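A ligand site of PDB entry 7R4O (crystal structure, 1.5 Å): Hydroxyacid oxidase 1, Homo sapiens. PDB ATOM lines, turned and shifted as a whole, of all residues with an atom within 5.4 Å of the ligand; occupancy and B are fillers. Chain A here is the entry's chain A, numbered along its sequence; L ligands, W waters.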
ATOM      1  N   TYR A  26      38.244  -0.391  21.487  1.00  0.00           N
ATOM      2  CA  TYR A  26      37.402  -0.057  22.649  1.00  0.00           C
ATOM      3  C   TYR A  26      36.261   0.862  22.206  1.00  0.00           C
ATOM      4  O   TYR A  26      35.123   0.677  22.627  1.00  0.00           O
ATOM      5  CB  TYR A  26      38.229   0.616  23.746  1.00  0.00           C
ATOM      6  CG  TYR A  26      37.346   1.269  24.773  1.00  0.00           C
ATOM      7  CD1 TYR A  26      36.602   0.496  25.653  1.00  0.00           C
ATOM      8  CD2 TYR A  26      37.177   2.639  24.802  1.00  0.00           C
ATOM      9  CE1 TYR A  26      35.750   1.080  26.562  1.00  0.00           C
ATOM     10  CE2 TYR A  26      36.325   3.232  25.708  1.00  0.00           C
ATOM     11  CZ  TYR A  26      35.612   2.459  26.592  1.00  0.00           C
ATOM     12  OH  TYR A  26      34.765   3.028  27.482  1.00  0.00           O
ATOM     13  N   TYR A  27      36.588   1.872  21.390  1.00  0.00           N
ATOM     14  CA  TYR A  27      35.565   2.868  20.987  1.00  0.00           C
ATOM     15  C   TYR A  27      34.647   2.303  19.897  1.00  0.00           C
ATOM     16  O   TYR A  27      33.441   2.598  19.944  1.00  0.00           O
ATOM     17  CB  TYR A  27      36.250   4.131  20.442  1.00  0.00           C
ATOM     18  CG  TYR A  27      37.021   4.932  21.460  1.00  0.00           C
ATOM     19  CD1 TYR A  27      36.425   5.370  22.626  1.00  0.00           C
ATOM     20  CD2 TYR A  27      38.351   5.263  21.256  1.00  0.00           C
ATOM     21  CE1 TYR A  27      37.113   6.116  23.571  1.00  0.00           C
ATOM     22  CE2 TYR A  27      39.057   6.015  22.185  1.00  0.00           C
ATOM     23  CZ  TYR A  27      38.439   6.443  23.347  1.00  0.00           C
ATOM     24  OH  TYR A  27      39.131   7.181  24.262  1.00  0.00           O
ATOM     25  N   ASN A  40      22.104  -0.274  13.828  1.00  0.00           N
ATOM     26  CA  ASN A  40      21.917   1.141  14.187  1.00  0.00           C
ATOM     27  C   ASN A  40      22.189   2.030  12.970  1.00  0.00           C
ATOM     28  O   ASN A  40      21.466   3.058  12.804  1.00  0.00           O
ATOM     29  CB  ASN A  40      22.824   1.575  15.329  1.00  0.00           C
ATOM     30  CG  ASN A  40      22.281   1.289  16.706  1.00  0.00           C
ATOM     31  OD1 ASN A  40      21.115   0.886  16.846  1.00  0.00           O
ATOM     32  ND2 ASN A  40      23.124   1.475  17.697  1.00  0.00           N
ATOM     33  N   GLY A  78      26.951  13.051  23.058  1.00  0.00           N
ATOM     34  CA  GLY A  78      26.627  12.019  24.045  1.00  0.00           C
ATOM     35  C   GLY A  78      27.818  11.622  24.886  1.00  0.00           C
ATOM     36  O   GLY A  78      28.960  11.821  24.482  1.00  0.00           O
ATOM     37  N   ALA A  79      27.544  10.956  26.002  1.00  0.00           N
ATOM     38  CA  ALA A  79      28.569  10.519  26.953  1.00  0.00           C
ATOM     39  C   ALA A  79      29.431   9.412  26.358  1.00  0.00           C
ATOM     40  O   ALA A  79      28.879   8.399  25.923  1.00  0.00           O
ATOM     41  CB  ALA A  79      27.931  10.073  28.240  1.00  0.00           C
ATOM     42  N   THR A  80      30.720   9.614  26.255  1.00  0.00           N
ATOM     43  CA  THR A  80      31.626   8.529  25.854  1.00  0.00           C
ATOM     44  C   THR A  80      32.775   8.550  26.854  1.00  0.00           C
ATOM     45  O   THR A  80      33.345   9.652  27.096  1.00  0.00           O
ATOM     46  CB  THR A  80      32.141   8.629  24.421  1.00  0.00           C
ATOM     47  OG1 THR A  80      32.590   9.964  24.187  1.00  0.00           O
ATOM     48  CG2 THR A  80      31.091   8.316  23.379  1.00  0.00           C
ATOM     49  N   ALA A  81      33.054   7.440  27.477  1.00  0.00           N
ATOM     50  CA  ALA A  81      34.043   7.332  28.553  1.00  0.00           C
ATOM     51  C   ALA A  81      35.443   7.587  28.034  1.00  0.00           C
ATOM     52  O   ALA A  81      35.749   7.290  26.894  1.00  0.00           O
ATOM     53  CB  ALA A  81      33.956   5.973  29.148  1.00  0.00           C
ATOM     54  N   MET A 106      26.989  16.049  27.047  1.00  0.00           N
ATOM     55  CA  MET A 106      26.678  15.085  28.111  1.00  0.00           C
ATOM     56  C   MET A 106      27.996  14.483  28.579  1.00  0.00           C
ATOM     57  O   MET A 106      28.661  13.764  27.807  1.00  0.00           O
ATOM     58  CB  MET A 106      25.727  14.020  27.560  1.00  0.00           C
ATOM     59  CG  MET A 106      25.251  13.091  28.655  1.00  0.00           C
ATOM     60  SD  MET A 106      24.576  11.514  28.028  1.00  0.00           S
ATOM     61  CE  MET A 106      23.345  12.124  26.855  1.00  0.00           C
ATOM     62  N   SER A 108      30.335  11.980  30.640  1.00  0.00           N
ATOM     63  CA  SER A 108      30.319  10.609  31.190  1.00  0.00           C
ATOM     64  C   SER A 108      30.653  10.570  32.676  1.00  0.00           C
ATOM     65  O   SER A 108      31.490  11.335  33.109  1.00  0.00           O
ATOM     66  CB  SER A 108      31.316   9.749  30.446  1.00  0.00           C
ATOM     67  OG  SER A 108      31.462   8.493  31.080  1.00  0.00           O
ATOM     68  N   SER A 109      29.985   9.672  33.388  1.00  0.00           N
ATOM     69  CA  SER A 109      30.374   9.417  34.793  1.00  0.00           C
ATOM     70  C   SER A 109      31.789   8.817  34.797  1.00  0.00           C
ATOM     71  O   SER A 109      32.466   8.932  35.812  1.00  0.00           O
ATOM     72  CB  SER A 109      29.383   8.470  35.455  1.00  0.00           C
ATOM     73  OG  SER A 109      28.444   9.192  36.237  1.00  0.00           O
ATOM     74  N   TRP A 110      32.218   8.233  33.682  1.00  0.00           N
ATOM     75  CA  TRP A 110      33.541   7.560  33.577  1.00  0.00           C
ATOM     76  C   TRP A 110      34.516   8.425  32.779  1.00  0.00           C
ATOM     77  O   TRP A 110      35.250   7.917  31.955  1.00  0.00           O
ATOM     78  CB  TRP A 110      33.371   6.210  32.908  1.00  0.00           C
ATOM     79  CG  TRP A 110      32.536   5.242  33.685  1.00  0.00           C
ATOM     80  CD1 TRP A 110      32.238   5.295  35.014  1.00  0.00           C
ATOM     81  CD2 TRP A 110      31.900   4.060  33.171  1.00  0.00           C
ATOM     82  NE1 TRP A 110      31.457   4.225  35.360  1.00  0.00           N
ATOM     83  CE2 TRP A 110      31.236   3.455  34.258  1.00  0.00           C
ATOM     84  CE3 TRP A 110      31.835   3.462  31.911  1.00  0.00           C
ATOM     85  CZ2 TRP A 110      30.504   2.279  34.112  1.00  0.00           C
ATOM     86  CZ3 TRP A 110      31.107   2.308  31.770  1.00  0.00           C
ATOM     87  CH2 TRP A 110      30.453   1.722  32.851  1.00  0.00           C
ATOM     88  N   GLN A 130      25.911  12.564  32.705  1.00  0.00           N
ATOM     89  CA  GLN A 130      25.438  11.157  32.665  1.00  0.00           C
ATOM     90  C   GLN A 130      25.881  10.447  33.938  1.00  0.00           C
ATOM     91  O   GLN A 130      27.043  10.592  34.319  1.00  0.00           O
ATOM     92  CB  GLN A 130      25.966  10.460  31.437  1.00  0.00           C
ATOM     93  CG  GLN A 130      25.650   8.973  31.347  1.00  0.00           C
ATOM     94  CD  GLN A 130      26.550   8.065  32.149  1.00  0.00           C
ATOM     95  OE1 GLN A 130      26.106   7.120  32.872  1.00  0.00           O
ATOM     96  NE2 GLN A 130      27.804   8.242  31.891  1.00  0.00           N
ATOM     97  N   TYR A 132      25.676   6.943  36.425  1.00  0.00           N
ATOM     98  CA  TYR A 132      25.436   5.541  36.803  1.00  0.00           C
ATOM     99  C   TYR A 132      25.094   5.547  38.278  1.00  0.00           C
ATOM    100  O   TYR A 132      25.754   6.349  39.018  1.00  0.00           O
ATOM    101  CB  TYR A 132      26.684   4.713  36.550  1.00  0.00           C
ATOM    102  CG  TYR A 132      26.943   4.351  35.121  1.00  0.00           C
ATOM    103  CD1 TYR A 132      26.002   3.576  34.451  1.00  0.00           C
ATOM    104  CD2 TYR A 132      28.032   4.800  34.410  1.00  0.00           C
ATOM    105  CE1 TYR A 132      26.185   3.234  33.139  1.00  0.00           C
ATOM    106  CE2 TYR A 132      28.231   4.462  33.074  1.00  0.00           C
ATOM    107  CZ  TYR A 132      27.299   3.639  32.465  1.00  0.00           C
ATOM    108  OH  TYR A 132      27.467   3.330  31.160  1.00  0.00           O
ATOM    109  N   THR A 158      21.701   6.466  33.232  1.00  0.00           N
ATOM    110  CA  THR A 158      21.816   5.297  32.331  1.00  0.00           C
ATOM    111  C   THR A 158      21.121   4.140  33.023  1.00  0.00           C
ATOM    112  O   THR A 158      21.512   3.807  34.183  1.00  0.00           O
ATOM    113  CB  THR A 158      23.278   5.062  31.970  1.00  0.00           C
ATOM    114  OG1 THR A 158      23.742   6.224  31.299  1.00  0.00           O
ATOM    115  CG2 THR A 158      23.389   3.862  31.066  1.00  0.00           C
ATOM    116  N   LYS A 236      18.130   7.233  30.205  1.00  0.00           N
ATOM    117  CA  LYS A 236      18.920   6.863  29.011  1.00  0.00           C
ATOM    118  C   LYS A 236      19.027   5.352  28.892  1.00  0.00           C
ATOM    119  O   LYS A 236      19.540   4.680  29.804  1.00  0.00           O
ATOM    120  CB  LYS A 236      20.294   7.483  29.132  1.00  0.00           C
ATOM    121  CG  LYS A 236      21.291   7.080  28.054  1.00  0.00           C
ATOM    122  CD  LYS A 236      22.610   7.831  28.243  1.00  0.00           C
ATOM    123  CE  LYS A 236      23.621   7.667  27.130  1.00  0.00           C
ATOM    124  NZ  LYS A 236      24.244   6.332  27.198  1.00  0.00           N
ATOM    125  N   SER A 258      18.005   4.648  23.371  1.00  0.00           N
ATOM    126  CA  SER A 258      19.425   4.324  23.282  1.00  0.00           C
ATOM    127  C   SER A 258      19.554   2.848  23.496  1.00  0.00           C
ATOM    128  O   SER A 258      18.866   2.313  24.394  1.00  0.00           O
ATOM    129  CB  SER A 258      20.220   5.118  24.275  1.00  0.00           C
ATOM    130  OG  SER A 258      21.605   4.745  24.236  1.00  0.00           O
ATOM    131  N   HIS A 260      22.766   2.021  23.941  1.00  0.00           N
ATOM    132  CA  HIS A 260      24.144   2.199  24.505  1.00  0.00           C
ATOM    133  C   HIS A 260      25.189   2.036  23.406  1.00  0.00           C
ATOM    134  O   HIS A 260      26.209   1.383  23.555  1.00  0.00           O
ATOM    135  CB  HIS A 260      24.344   1.227  25.663  1.00  0.00           C
ATOM    136  CG  HIS A 260      25.346   1.665  26.666  1.00  0.00           C
ATOM    137  ND1 HIS A 260      25.006   1.766  28.015  1.00  0.00           N
ATOM    138  CD2 HIS A 260      26.709   1.829  26.586  1.00  0.00           C
ATOM    139  CE1 HIS A 260      26.141   2.109  28.673  1.00  0.00           C
ATOM    140  NE2 HIS A 260      27.185   2.101  27.844  1.00  0.00           N
ATOM    141  N   GLY A 261      24.916   2.529  22.204  1.00  0.00           N
ATOM    142  CA  GLY A 261      25.789   2.412  21.050  1.00  0.00           C
ATOM    143  C   GLY A 261      26.017   0.948  20.713  1.00  0.00           C
ATOM    144  O   GLY A 261      27.046   0.573  20.158  1.00  0.00           O
ATOM    145  N   ARG A 263      26.338  -1.612  22.668  1.00  0.00           N
ATOM    146  CA  ARG A 263      27.458  -2.194  23.451  1.00  0.00           C
ATOM    147  C   ARG A 263      26.946  -2.983  24.659  1.00  0.00           C
ATOM    148  O   ARG A 263      27.779  -3.480  25.406  1.00  0.00           O
ATOM    149  CB  ARG A 263      28.368  -1.054  23.921  1.00  0.00           C
ATOM    150  CG  ARG A 263      29.146  -0.386  22.814  1.00  0.00           C
ATOM    151  CD  ARG A 263      29.593   1.005  23.220  1.00  0.00           C
ATOM    152  NE  ARG A 263      30.726   1.058  24.132  1.00  0.00           N
ATOM    153  CZ  ARG A 263      31.992   0.914  23.775  1.00  0.00           C
ATOM    154  NH1 ARG A 263      32.307   0.662  22.518  1.00  0.00           N
ATOM    155  NH2 ARG A 263      32.951   1.012  24.675  1.00  0.00           N
ATOM    156  N   ASP A 291      19.961   8.293  20.373  1.00  0.00           N
ATOM    157  CA  ASP A 291      21.357   8.121  19.961  1.00  0.00           C
ATOM    158  C   ASP A 291      21.475   6.743  19.357  1.00  0.00           C
ATOM    159  O   ASP A 291      20.548   5.899  19.456  1.00  0.00           O
ATOM    160  CB  ASP A 291      22.332   8.397  21.101  1.00  0.00           C
ATOM    161  CG  ASP A 291      22.363   7.435  22.232  1.00  0.00           C
ATOM    162  OD1 ASP A 291      21.956   6.271  22.060  1.00  0.00           O
ATOM    163  OD2 ASP A 291      22.822   7.821  23.311  1.00  0.00           O
ATOM    164  N   GLY A 292      22.619   6.478  18.720  1.00  0.00           N
ATOM    165  CA  GLY A 292      22.914   5.191  18.139  1.00  0.00           C
ATOM    166  C   GLY A 292      22.909   5.283  16.628  1.00  0.00           C
ATOM    167  O   GLY A 292      21.803   5.231  16.035  1.00  0.00           O
ATOM    168  N   GLY A 293      24.072   5.327  16.001  1.00  0.00           N
ATOM    169  CA  GLY A 293      24.181   5.267  14.560  1.00  0.00           C
ATOM    170  C   GLY A 293      24.033   6.595  13.837  1.00  0.00           C
ATOM    171  O   GLY A 293      23.998   6.571  12.621  1.00  0.00           O
ATOM    172  N   VAL A 294      23.972   7.712  14.527  1.00  0.00           N
ATOM    173  CA  VAL A 294      23.861   9.027  13.841  1.00  0.00           C
ATOM    174  C   VAL A 294      25.235   9.370  13.256  1.00  0.00           C
ATOM    175  O   VAL A 294      26.215   9.568  14.013  1.00  0.00           O
ATOM    176  CB  VAL A 294      23.336  10.116  14.771  1.00  0.00           C
ATOM    177  CG1 VAL A 294      23.381  11.455  14.085  1.00  0.00           C
ATOM    178  CG2 VAL A 294      21.951   9.772  15.306  1.00  0.00           C
ATOM    179  N   ARG A 295      25.302   9.473  11.936  1.00  0.00           N
ATOM    180  CA  ARG A 295      26.550   9.759  11.214  1.00  0.00           C
ATOM    181  C   ARG A 295      26.371  10.857  10.203  1.00  0.00           C
ATOM    182  O   ARG A 295      27.378  11.379   9.748  1.00  0.00           O
ATOM    183  CB  ARG A 295      27.031   8.493  10.533  1.00  0.00           C
ATOM    184  CG  ARG A 295      27.275   7.291  11.416  1.00  0.00           C
ATOM    185  CD  ARG A 295      28.370   7.443  12.398  1.00  0.00           C
ATOM    186  NE  ARG A 295      28.480   6.273  13.263  1.00  0.00           N
ATOM    187  CZ  ARG A 295      28.025   6.176  14.494  1.00  0.00           C
ATOM    188  NH1 ARG A 295      27.411   7.172  15.098  1.00  0.00           N
ATOM    189  NH2 ARG A 295      28.259   5.064  15.191  1.00  0.00           N
ATOM    190  N   PHE A 312      21.843  12.585  19.937  1.00  0.00           N
ATOM    191  CA  PHE A 312      23.190  12.585  20.528  1.00  0.00           C
ATOM    192  C   PHE A 312      24.117  11.748  19.689  1.00  0.00           C
ATOM    193  O   PHE A 312      23.711  10.720  19.130  1.00  0.00           O
ATOM    194  CB  PHE A 312      23.198  12.099  21.978  1.00  0.00           C
ATOM    195  CG  PHE A 312      22.438  13.001  22.900  1.00  0.00           C
ATOM    196  CD1 PHE A 312      21.044  12.960  22.971  1.00  0.00           C
ATOM    197  CD2 PHE A 312      23.087  13.945  23.674  1.00  0.00           C
ATOM    198  CE1 PHE A 312      20.330  13.871  23.722  1.00  0.00           C
ATOM    199  CE2 PHE A 312      22.361  14.798  24.483  1.00  0.00           C
ATOM    200  CZ  PHE A 312      21.001  14.759  24.524  1.00  0.00           C
ATOM    201  N   VAL A 313      25.358  12.190  19.596  1.00  0.00           N
ATOM    202  CA  VAL A 313      26.387  11.444  18.861  1.00  0.00           C
ATOM    203  C   VAL A 313      27.430  10.986  19.855  1.00  0.00           C
ATOM    204  O   VAL A 313      27.911  11.811  20.663  1.00  0.00           O
ATOM    205  CB  VAL A 313      26.982  12.242  17.705  1.00  0.00           C
ATOM    206  CG1 VAL A 313      25.991  12.252  16.515  1.00  0.00           C
ATOM    207  CG2 VAL A 313      27.398  13.587  18.129  1.00  0.00           C
ATOM    208  N   GLY A 314      27.851   9.733  19.710  1.00  0.00           N
ATOM    209  CA  GLY A 314      28.856   9.136  20.586  1.00  0.00           C
ATOM    210  C   GLY A 314      30.169   9.036  19.851  1.00  0.00           C
ATOM    211  O   GLY A 314      31.022   9.960  19.952  1.00  0.00           O
ATOM    212  N   ARG A 315      30.378   7.991  19.100  1.00  0.00           N
ATOM    213  CA  ARG A 315      31.673   7.689  18.467  1.00  0.00           C
ATOM    214  C   ARG A 315      32.188   8.826  17.611  1.00  0.00           C
ATOM    215  O   ARG A 315      33.398   9.036  17.661  1.00  0.00           O
ATOM    216  CB  ARG A 315      31.568   6.386  17.699  1.00  0.00           C
ATOM    217  CG  ARG A 315      31.462   5.157  18.585  1.00  0.00           C
ATOM    218  CD  ARG A 315      31.285   3.902  17.750  1.00  0.00           C
ATOM    219  NE  ARG A 315      31.044   2.733  18.602  1.00  0.00           N
ATOM    220  CZ  ARG A 315      29.843   2.293  18.979  1.00  0.00           C
ATOM    221  NH1 ARG A 315      28.761   2.955  18.631  1.00  0.00           N
ATOM    222  NH2 ARG A 315      29.771   1.128  19.612  1.00  0.00           N
ATOM    223  N   PRO A 316      31.390   9.514  16.803  1.00  0.00           N
ATOM    224  CA  PRO A 316      31.951  10.550  15.917  1.00  0.00           C
ATOM    225  C   PRO A 316      32.764  11.581  16.697  1.00  0.00           C
ATOM    226  O   PRO A 316      33.743  12.096  16.165  1.00  0.00           O
ATOM    227  CB  PRO A 316      30.733  11.142  15.249  1.00  0.00           C
ATOM    228  CG  PRO A 316      29.826   9.924  15.112  1.00  0.00           C
ATOM    229  CD  PRO A 316      29.951   9.304  16.491  1.00  0.00           C
ATOM    230  N   VAL A 318      34.566  11.087  19.444  1.00  0.00           N
ATOM    231  CA  VAL A 318      35.868  10.449  19.756  1.00  0.00           C
ATOM    232  C   VAL A 318      36.723  10.484  18.499  1.00  0.00           C
ATOM    233  O   VAL A 318      37.976  10.733  18.594  1.00  0.00           O
ATOM    234  CB  VAL A 318      35.636   9.027  20.273  1.00  0.00           C
ATOM    235  CG1 VAL A 318      36.978   8.406  20.572  1.00  0.00           C
ATOM    236  CG2 VAL A 318      34.753   9.081  21.506  1.00  0.00           C
HETATM  237  N1  LIG L   1      27.109   5.634  27.738  1.00  0.00           N
HETATM  238  C1  LIG L   1      27.045   6.089  28.985  1.00  0.00           C
HETATM  239  O1  LIG L   1      25.955   6.212  29.548  1.00  0.00           O
HETATM  240  N2  LIG L   1      28.167   6.365  29.703  1.00  0.00           N
HETATM  241  C2  LIG L   1      29.426   6.072  29.234  1.00  0.00           C
HETATM  242  O2  LIG L   1      30.390   6.387  29.917  1.00  0.00           O
HETATM  243  C3  LIG L   1      29.533   5.616  27.903  1.00  0.00           C
HETATM  244  N3  LIG L   1      30.734   5.402  27.366  1.00  0.00           N
HETATM  245  C4  LIG L   1      30.783   5.026  26.062  1.00  0.00           C
HETATM  246  C5  LIG L   1      32.037   4.840  25.476  1.00  0.00           C
HETATM  247  C6  LIG L   1      32.157   4.499  24.158  1.00  0.00           C
HETATM  248  C7  LIG L   1      33.511   4.353  23.540  1.00  0.00           C
HETATM  249  C8  LIG L   1      31.006   4.422  23.361  1.00  0.00           C
HETATM  250  C9  LIG L   1      31.137   4.107  21.888  1.00  0.00           C
HETATM  251  C10 LIG L   1      29.747   4.604  23.928  1.00  0.00           C
HETATM  252  C11 LIG L   1      29.600   4.894  25.285  1.00  0.00           C
HETATM  253  N4  LIG L   1      28.360   5.083  25.888  1.00  0.00           N
HETATM  254  C12 LIG L   1      28.294   5.463  27.206  1.00  0.00           C
HETATM  255  C13 LIG L   1      27.106   5.096  25.106  1.00  0.00           C
HETATM  256  C14 LIG L   1      26.934   6.479  24.439  1.00  0.00           C
HETATM  257  O3  LIG L   1      26.445   7.440  25.400  1.00  0.00           O
HETATM  258  C15 LIG L   1      25.883   6.513  23.342  1.00  0.00           C
HETATM  259  O4  LIG L   1      24.668   5.855  23.792  1.00  0.00           O
HETATM  260  C16 LIG L   1      26.353   5.840  22.069  1.00  0.00           C
HETATM  261  O5  LIG L   1      27.756   6.140  21.833  1.00  0.00           O
HETATM  262  C17 LIG L   1      25.562   6.329  20.894  1.00  0.00           C
HETATM  263  O6  LIG L   1      25.832   5.659  19.646  1.00  0.00           O
HETATM  264  P1  LIG L   1      26.940   6.175  18.560  1.00  0.00           P
HETATM  265  O7  LIG L   1      26.744   7.609  18.244  1.00  0.00           O
HETATM  266  O8  LIG L   1      28.329   5.892  19.129  1.00  0.00           O
HETATM  267  O9  LIG L   1      26.581   5.264  17.448  1.00  0.00           O
HETATM  268  O   HOH W   1      25.836   2.593  17.627  1.00  0.00           O
HETATM  269  O   HOH W   2      24.294   8.427  17.624  1.00  0.00           O
HETATM  270  O   HOH W   3      24.653   9.589  24.519  1.00  0.00           O
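The guanidinium group (NH2) of Arg 295 lies within salt-bridge range of an oxygen (O9) of the ligand (2.8 Å). An oxygen (O4) of the ligand is in hydrogen-bond range of the side-chain hydroxyl of Ser 258 (3.3 Å). An oxygen (O6) of the ligand lies close to the backbone NH of Gly 292 (3.4 Å). The backbone NH (N) of Arg 315 sits at hydrogen-bond distance from an oxygen (O8) of the ligand (2.9 Å). An oxygen (O4) of the ligand is in hydrogen-bond range of the side-chain carboxylate of Asp 291, at 2.7 Å. O7 of the ligand sits at hydrogen-bond distance from N of Gly 314, 2.8 Å away. An oxygen (O8) of the ligand is in salt-bridge range of the guanidinium group (NH1) of Arg 315. The side-chain hydroxyl (OG) of Ser 108 sits at hydrogen-bond distance from an oxygen (O2) of the ligand, at 2.6 Å. The side-chain hydroxyl (OG1) of Thr 158 is in hydrogen-bond range of an oxygen (O1) of the ligand. The side-chain amino group (NZ) of Lys 236 lies within hydrogen-bond range of an oxygen (O1) of the ligand (2.9 Å). O9 of the ligand sits at hydrogen-bond distance from N of Gly 293 (2.9 Å). A nitrogen (N2) of the ligand lies close to the side-chain amide nitrogen (NE2) of Gln 130 (2.9 Å). A nitrogen (N2) of the ligand lies within hydrogen-bond range of the side-chain hydroxyl (OH) of Tyr 132 (3.4 Å). The backbone carbonyl oxygen (O) of Ala 79 sits at hydrogen-bond distance from an oxygen (O3) of the ligand (2.7 Å). The backbone NH of Ala 81 is in hydrogen-bond range of a nitrogen (N3) of the ligand (3.1 Å).
The backbone NH (N) of His 260 lies within hydrogen-bond range of the side-chain hydroxyl (OG) of Ser 258 (3.0 Å). OG1 of Thr 158 lies within hydrogen-bond range of OE1 of Gln 130 (3.0 Å). The guanidinium group (NE) of Arg 315 is in hydrogen-bond range of the backbone carbonyl oxygen (O) of Tyr 27 (2.8 Å). OD1 of Asp 291 lies within hydrogen-bond range of OG of Ser 258, at 2.7 Å. The side-chain hydroxyl (OG) of Ser 108 is in hydrogen-bond range of the backbone NH (N) of Trp 110. The guanidinium group (NH2) of Arg 315 is in hydrogen-bond range of the backbone carbonyl oxygen (O) of Gly 261, 2.8 Å away. O of Gln 130 sits at hydrogen-bond distance from OG of Ser 109. The backbone NH (N) of Ala 79 sits at hydrogen-bond distance from the side-chain sulfur (SD) of Met 106 (3.6 Å).
CE2 of Tyr 26 touches C7 of the ligand (3.7 Å). Tyr 27 touches the ligand. CA of Thr 80 touches N3 of the ligand, 3.6 Å away. Trp 110 touches the ligand. His 260 touches the ligand. CA of Gly 261 touches O6 of the ligand, at 3.5 Å. Arg 263 touches the ligand. C of Val 313 touches O7 of the ligand, 3.8 Å away. The nearest printed residue that does not touch the ligand is Pro 316 (4.03 Å).
Water W2 lies within hydrogen-bond range of an oxygen (O7) of the ligand (2.7 Å), the backbone NH of Gly 292 (2.8 Å), the backbone carbonyl oxygen of Phe 312 (2.8 Å) and the backbone NH of Val 294 (3.2 Å). Water W1 lies within hydrogen-bond range of an oxygen (O9) of the ligand (2.8 Å), the side-chain amide nitrogen (ND2) of Asn 40 (2.9 Å), the guanidinium group (NH1) of Arg 315 (3.1 Å) and the backbone carbonyl oxygen (O) of Gly 261 (3.5 Å). Water W3 bridges the side-chain carboxylate of Asp 291 and an oxygen (O3) of the ligand.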
